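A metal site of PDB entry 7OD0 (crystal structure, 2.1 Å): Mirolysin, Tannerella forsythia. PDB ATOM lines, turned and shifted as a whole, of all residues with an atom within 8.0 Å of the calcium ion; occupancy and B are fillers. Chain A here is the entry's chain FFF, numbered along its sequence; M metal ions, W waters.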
ATOM      1  N   HIS A 180     -13.843 -26.858 -22.851  1.00  0.00           N
ATOM      2  CA  HIS A 180     -13.628 -26.778 -24.322  1.00  0.00           C
ATOM      3  C   HIS A 180     -12.999 -25.424 -24.665  1.00  0.00           C
ATOM      4  O   HIS A 180     -13.528 -24.368 -24.201  1.00  0.00           O
ATOM      5  CB  HIS A 180     -14.936 -26.994 -25.087  1.00  0.00           C
ATOM      6  CG  HIS A 180     -15.425 -28.385 -24.962  1.00  0.00           C
ATOM      7  ND1 HIS A 180     -16.758 -28.684 -24.892  1.00  0.00           N
ATOM      8  CD2 HIS A 180     -14.769 -29.565 -24.914  1.00  0.00           C
ATOM      9  CE1 HIS A 180     -16.910 -29.988 -24.819  1.00  0.00           C
ATOM     10  NE2 HIS A 180     -15.707 -30.556 -24.830  1.00  0.00           N
ATOM     11  N   ILE A 181     -11.940 -25.460 -25.465  1.00  0.00           N
ATOM     12  CA  ILE A 181     -11.087 -24.285 -25.781  1.00  0.00           C
ATOM     13  C   ILE A 181     -11.923 -23.196 -26.465  1.00  0.00           C
ATOM     14  O   ILE A 181     -11.550 -22.026 -26.325  1.00  0.00           O
ATOM     15  CB  ILE A 181      -9.879 -24.700 -26.637  1.00  0.00           C
ATOM     16  CG1 ILE A 181      -8.863 -23.566 -26.798  1.00  0.00           C
ATOM     17  CG2 ILE A 181     -10.309 -25.260 -27.984  1.00  0.00           C
ATOM     18  CD1 ILE A 181      -7.539 -24.023 -27.341  1.00  0.00           C
ATOM     19  N   TRP A 182     -12.998 -23.550 -27.171  1.00  0.00           N
ATOM     20  CA  TRP A 182     -13.843 -22.595 -27.935  1.00  0.00           C
ATOM     21  C   TRP A 182     -14.944 -21.995 -27.020  1.00  0.00           C
ATOM     22  O   TRP A 182     -15.621 -21.059 -27.453  1.00  0.00           O
ATOM     23  CB  TRP A 182     -14.399 -23.278 -29.208  1.00  0.00           C
ATOM     24  CG  TRP A 182     -15.458 -24.294 -28.949  1.00  0.00           C
ATOM     25  CD1 TRP A 182     -16.804 -24.065 -28.873  1.00  0.00           C
ATOM     26  CD2 TRP A 182     -15.286 -25.699 -28.699  1.00  0.00           C
ATOM     27  NE1 TRP A 182     -17.465 -25.221 -28.576  1.00  0.00           N
ATOM     28  CE2 TRP A 182     -16.566 -26.252 -28.475  1.00  0.00           C
ATOM     29  CE3 TRP A 182     -14.189 -26.568 -28.657  1.00  0.00           C
ATOM     30  CZ2 TRP A 182     -16.774 -27.601 -28.211  1.00  0.00           C
ATOM     31  CZ3 TRP A 182     -14.387 -27.906 -28.376  1.00  0.00           C
ATOM     32  CH2 TRP A 182     -15.663 -28.407 -28.165  1.00  0.00           C
ATOM     33  N   GLY A 183     -15.127 -22.519 -25.809  1.00  0.00           N
ATOM     34  CA  GLY A 183     -16.002 -21.894 -24.803  1.00  0.00           C
ATOM     35  C   GLY A 183     -17.440 -22.394 -24.849  1.00  0.00           C
ATOM     36  O   GLY A 183     -18.308 -21.732 -24.255  1.00  0.00           O
ATOM     37  N   ASP A 184     -17.725 -23.501 -25.529  1.00  0.00           N
ATOM     38  CA  ASP A 184     -19.080 -24.106 -25.483  1.00  0.00           C
ATOM     39  C   ASP A 184     -20.128 -23.027 -25.821  1.00  0.00           C
ATOM     40  O   ASP A 184     -21.121 -22.919 -25.097  1.00  0.00           O
ATOM     41  CB  ASP A 184     -19.332 -24.755 -24.118  1.00  0.00           C
ATOM     42  CG  ASP A 184     -18.443 -25.966 -23.867  1.00  0.00           C
ATOM     43  OD1 ASP A 184     -18.404 -26.812 -24.749  1.00  0.00           O
ATOM     44  OD2 ASP A 184     -17.770 -26.041 -22.837  1.00  0.00           O
ATOM     45  N   ASP A 185     -19.924 -22.273 -26.884  1.00  0.00           N
ATOM     46  CA  ASP A 185     -20.799 -21.130 -27.232  1.00  0.00           C
ATOM     47  C   ASP A 185     -21.304 -21.272 -28.671  1.00  0.00           C
ATOM     48  O   ASP A 185     -21.756 -20.240 -29.238  1.00  0.00           O
ATOM     49  CB  ASP A 185     -20.056 -19.818 -27.008  1.00  0.00           C
ATOM     50  CG  ASP A 185     -18.740 -19.733 -27.749  1.00  0.00           C
ATOM     51  OD1 ASP A 185     -18.549 -20.527 -28.727  1.00  0.00           O
ATOM     52  OD2 ASP A 185     -17.893 -18.880 -27.373  1.00  0.00           O
ATOM     53  N   GLY A 186     -21.247 -22.488 -29.223  1.00  0.00           N
ATOM     54  CA  GLY A 186     -21.836 -22.825 -30.524  1.00  0.00           C
ATOM     55  C   GLY A 186     -21.218 -22.041 -31.678  1.00  0.00           C
ATOM     56  O   GLY A 186     -21.864 -21.947 -32.707  1.00  0.00           O
ATOM     57  N   GLY A 187     -20.039 -21.438 -31.495  1.00  0.00           N
ATOM     58  CA  GLY A 187     -19.308 -20.764 -32.585  1.00  0.00           C
ATOM     59  C   GLY A 187     -19.033 -19.282 -32.345  1.00  0.00           C
ATOM     60  O   GLY A 187     -18.256 -18.729 -33.148  1.00  0.00           O
ATOM     61  N   SER A 188     -19.615 -18.644 -31.308  1.00  0.00           N
ATOM     62  CA  SER A 188     -19.463 -17.171 -31.091  1.00  0.00           C
ATOM     63  C   SER A 188     -18.062 -16.902 -30.568  1.00  0.00           C
ATOM     64  O   SER A 188     -17.310 -17.870 -30.377  1.00  0.00           O
ATOM     65  CB  SER A 188     -20.494 -16.625 -30.135  1.00  0.00           C
ATOM     66  OG  SER A 188     -20.213 -17.063 -28.818  1.00  0.00           O
ATOM     67  N   CYS A 189     -17.754 -15.635 -30.315  1.00  0.00           N
ATOM     68  CA  CYS A 189     -16.513 -15.190 -29.631  1.00  0.00           C
ATOM     69  C   CYS A 189     -16.792 -14.889 -28.145  1.00  0.00           C
ATOM     70  O   CYS A 189     -15.832 -14.525 -27.449  1.00  0.00           O
ATOM     71  CB  CYS A 189     -15.960 -13.972 -30.342  1.00  0.00           C
ATOM     72  SG  CYS A 189     -15.697 -14.303 -32.110  1.00  0.00           S
ATOM     73  N   SER A 190     -18.024 -15.079 -27.680  1.00  0.00           N
ATOM     74  CA  SER A 190     -18.502 -14.616 -26.338  1.00  0.00           C
ATOM     75  C   SER A 190     -18.048 -15.558 -25.224  1.00  0.00           C
ATOM     76  O   SER A 190     -17.580 -15.053 -24.190  1.00  0.00           O
ATOM     77  CB  SER A 190     -20.003 -14.428 -26.284  1.00  0.00           C
ATOM     78  OG  SER A 190     -20.359 -13.244 -26.968  1.00  0.00           O
ATOM     79  N   GLY A 191     -18.264 -16.865 -25.399  1.00  0.00           N
ATOM     80  CA  GLY A 191     -17.828 -17.899 -24.436  1.00  0.00           C
ATOM     81  C   GLY A 191     -16.325 -17.897 -24.203  1.00  0.00           C
ATOM     82  O   GLY A 191     -15.583 -17.404 -25.064  1.00  0.00           O
ATOM     83  N   THR A 192     -15.886 -18.432 -23.073  1.00  0.00           N
ATOM     84  CA  THR A 192     -14.461 -18.504 -22.670  1.00  0.00           C
ATOM     85  C   THR A 192     -14.218 -19.863 -22.001  1.00  0.00           C
ATOM     86  O   THR A 192     -15.134 -20.365 -21.340  1.00  0.00           O
ATOM     87  CB  THR A 192     -14.110 -17.357 -21.714  1.00  0.00           C
ATOM     88  OG1 THR A 192     -12.746 -17.533 -21.373  1.00  0.00           O
ATOM     89  CG2 THR A 192     -14.924 -17.303 -20.436  1.00  0.00           C
ATOM     90  N   ASP A 193     -13.002 -20.375 -22.135  1.00  0.00           N
ATOM     91  CA  ASP A 193     -12.516 -21.553 -21.372  1.00  0.00           C
ATOM     92  C   ASP A 193     -11.811 -21.081 -20.092  1.00  0.00           C
ATOM     93  O   ASP A 193     -11.301 -21.939 -19.346  1.00  0.00           O
ATOM     94  CB  ASP A 193     -11.608 -22.424 -22.266  1.00  0.00           C
ATOM     95  CG  ASP A 193     -10.307 -21.757 -22.663  1.00  0.00           C
ATOM     96  OD1 ASP A 193     -10.179 -20.536 -22.474  1.00  0.00           O
ATOM     97  OD2 ASP A 193      -9.426 -22.479 -23.152  1.00  0.00           O
ATOM     98  N   PRO A 199      -5.937 -18.925 -27.341  1.00  0.00           N
ATOM     99  CA  PRO A 199      -6.525 -17.857 -28.131  1.00  0.00           C
ATOM    100  C   PRO A 199      -8.045 -18.029 -28.236  1.00  0.00           C
ATOM    101  O   PRO A 199      -8.513 -19.159 -28.291  1.00  0.00           O
ATOM    102  CB  PRO A 199      -5.905 -18.011 -29.530  1.00  0.00           C
ATOM    103  CG  PRO A 199      -4.634 -18.816 -29.293  1.00  0.00           C
ATOM    104  CD  PRO A 199      -4.945 -19.716 -28.098  1.00  0.00           C
ATOM    105  N   ASN A 200      -8.780 -16.923 -28.229  1.00  0.00           N
ATOM    106  CA  ASN A 200     -10.263 -16.911 -28.376  1.00  0.00           C
ATOM    107  C   ASN A 200     -10.586 -17.670 -29.674  1.00  0.00           C
ATOM    108  O   ASN A 200      -9.847 -17.523 -30.672  1.00  0.00           O
ATOM    109  CB  ASN A 200     -10.840 -15.496 -28.363  1.00  0.00           C
ATOM    110  CG  ASN A 200     -12.335 -15.503 -28.106  1.00  0.00           C
ATOM    111  OD1 ASN A 200     -12.872 -16.490 -27.606  1.00  0.00           O
ATOM    112  ND2 ASN A 200     -13.025 -14.408 -28.419  1.00  0.00           N
ATOM    113  N   GLN A 201     -11.648 -18.447 -29.668  1.00  0.00           N
ATOM    114  CA  GLN A 201     -11.945 -19.371 -30.782  1.00  0.00           C
ATOM    115  C   GLN A 201     -13.461 -19.468 -30.945  1.00  0.00           C
ATOM    116  O   GLN A 201     -14.154 -19.574 -29.912  1.00  0.00           O
ATOM    117  CB  GLN A 201     -11.247 -20.700 -30.480  1.00  0.00           C
ATOM    118  CG  GLN A 201     -11.665 -21.850 -31.382  1.00  0.00           C
ATOM    119  CD  GLN A 201     -10.886 -23.114 -31.131  1.00  0.00           C
ATOM    120  OE1 GLN A 201      -9.747 -23.126 -30.661  1.00  0.00           O
ATOM    121  NE2 GLN A 201     -11.526 -24.224 -31.444  1.00  0.00           N
ATOM    122  N   GLY A 202     -13.959 -19.453 -32.186  1.00  0.00           N
ATOM    123  CA  GLY A 202     -15.402 -19.497 -32.490  1.00  0.00           C
ATOM    124  C   GLY A 202     -15.983 -20.833 -32.068  1.00  0.00           C
ATOM    125  O   GLY A 202     -16.574 -20.929 -30.978  1.00  0.00           O
ATOM    126  N   GLY A 203     -15.810 -21.844 -32.917  1.00  0.00           N
ATOM    127  CA  GLY A 203     -16.393 -23.164 -32.691  1.00  0.00           C
ATOM    128  C   GLY A 203     -15.313 -24.187 -32.512  1.00  0.00           C
ATOM    129  O   GLY A 203     -14.130 -23.809 -32.550  1.00  0.00           O
ATOM    130  N   TYR A 204     -15.719 -25.437 -32.333  1.00  0.00           N
ATOM    131  CA  TYR A 204     -14.790 -26.588 -32.212  1.00  0.00           C
ATOM    132  C   TYR A 204     -14.174 -26.864 -33.576  1.00  0.00           C
ATOM    133  O   TYR A 204     -14.775 -26.520 -34.612  1.00  0.00           O
ATOM    134  CB  TYR A 204     -15.484 -27.830 -31.658  1.00  0.00           C
ATOM    135  CG  TYR A 204     -16.659 -28.357 -32.447  1.00  0.00           C
ATOM    136  CD1 TYR A 204     -16.476 -29.132 -33.590  1.00  0.00           C
ATOM    137  CD2 TYR A 204     -17.951 -28.159 -32.004  1.00  0.00           C
ATOM    138  CE1 TYR A 204     -17.565 -29.635 -34.286  1.00  0.00           C
ATOM    139  CE2 TYR A 204     -19.045 -28.659 -32.692  1.00  0.00           C
ATOM    140  CZ  TYR A 204     -18.851 -29.409 -33.835  1.00  0.00           C
ATOM    141  OH  TYR A 204     -19.969 -29.898 -34.467  1.00  0.00           O
ATOM    142  N   ASP A 215     -10.356 -17.829 -37.467  1.00  0.00           N
ATOM    143  CA  ASP A 215     -11.833 -17.667 -37.478  1.00  0.00           C
ATOM    144  C   ASP A 215     -12.130 -16.203 -37.150  1.00  0.00           C
ATOM    145  O   ASP A 215     -11.167 -15.415 -36.988  1.00  0.00           O
ATOM    146  CB  ASP A 215     -12.522 -18.674 -36.548  1.00  0.00           C
ATOM    147  CG  ASP A 215     -12.207 -18.558 -35.059  1.00  0.00           C
ATOM    148  OD1 ASP A 215     -11.817 -17.457 -34.607  1.00  0.00           O
ATOM    149  OD2 ASP A 215     -12.348 -19.591 -34.361  1.00  0.00           O
ATOM    150  N   HIS A 216     -13.403 -15.843 -37.036  1.00  0.00           N
ATOM    151  CA  HIS A 216     -13.808 -14.425 -36.811  1.00  0.00           C
ATOM    152  C   HIS A 216     -13.330 -13.940 -35.432  1.00  0.00           C
ATOM    153  O   HIS A 216     -13.246 -12.723 -35.274  1.00  0.00           O
ATOM    154  CB  HIS A 216     -15.308 -14.213 -37.056  1.00  0.00           C
ATOM    155  CG  HIS A 216     -16.246 -14.891 -36.115  1.00  0.00           C
ATOM    156  ND1 HIS A 216     -17.134 -14.175 -35.311  1.00  0.00           N
ATOM    157  CD2 HIS A 216     -16.518 -16.190 -35.900  1.00  0.00           C
ATOM    158  CE1 HIS A 216     -17.881 -15.010 -34.628  1.00  0.00           C
ATOM    159  NE2 HIS A 216     -17.533 -16.242 -34.978  1.00  0.00           N
ATOM    160  N   CYS A 217     -12.973 -14.840 -34.504  1.00  0.00           N
ATOM    161  CA  CYS A 217     -12.506 -14.497 -33.127  1.00  0.00           C
ATOM    162  C   CYS A 217     -11.002 -14.240 -33.098  1.00  0.00           C
ATOM    163  O   CYS A 217     -10.598 -13.299 -32.422  1.00  0.00           O
ATOM    164  CB  CYS A 217     -12.838 -15.587 -32.117  1.00  0.00           C
ATOM    165  SG  CYS A 217     -14.583 -16.056 -32.166  1.00  0.00           S
HETATM  166 CA    CA M   1     -16.408 -19.497 -29.010  1.00  0.00          CA
HETATM  167  O   HOH W   1     -15.001 -17.993 -27.793  1.00  0.00           O
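Water W1 lies within hydrogen-bond range of the side-chain amide oxygen of Asn 200 (2.6 Å) and the backbone carbonyl oxygen of Gly 191 (2.9 Å).
The calcium ion is bound by OD2 of Asp 185 (2.3 Å), O of Ser 188 (2.3 Å), O of Trp 182 (2.3 Å), water W1 (2.4 Å), OD1 of Asp 185 (2.4 Å), O of Gln 201 (2.4 Å) and O of Gly 202 (2.4 Å). The calcium ion has seven donor atoms within binding distance.
The backbone NH of Gly 187 lies close to the side-chain carboxylate of Asp 185 (3.3 Å). OD2 of Asp 185 sits close to N of Gly 191 (2.8 Å). OG of Ser 188 sits at hydrogen-bond distance from N of Ser 190. The side-chain amide nitrogen (NE2) of Gln 201 is in hydrogen-bond range of the backbone carbonyl oxygen (O) of Gly 203 (2.9 Å). The backbone NH (N) of Gly 202 is in hydrogen-bond range of the side-chain sulfur (SG) of Cys 217 (3.5 Å). The backbone NH (N) of Gly 202 is in hydrogen-bond range of the side-chain carboxylate (OD2) of Asp 215 (2.7 Å). The side-chain sulfur (SG) of Cys 189 forms a disulfide with the side-chain sulfur (SG) of Cys 217 (2.1 Å).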
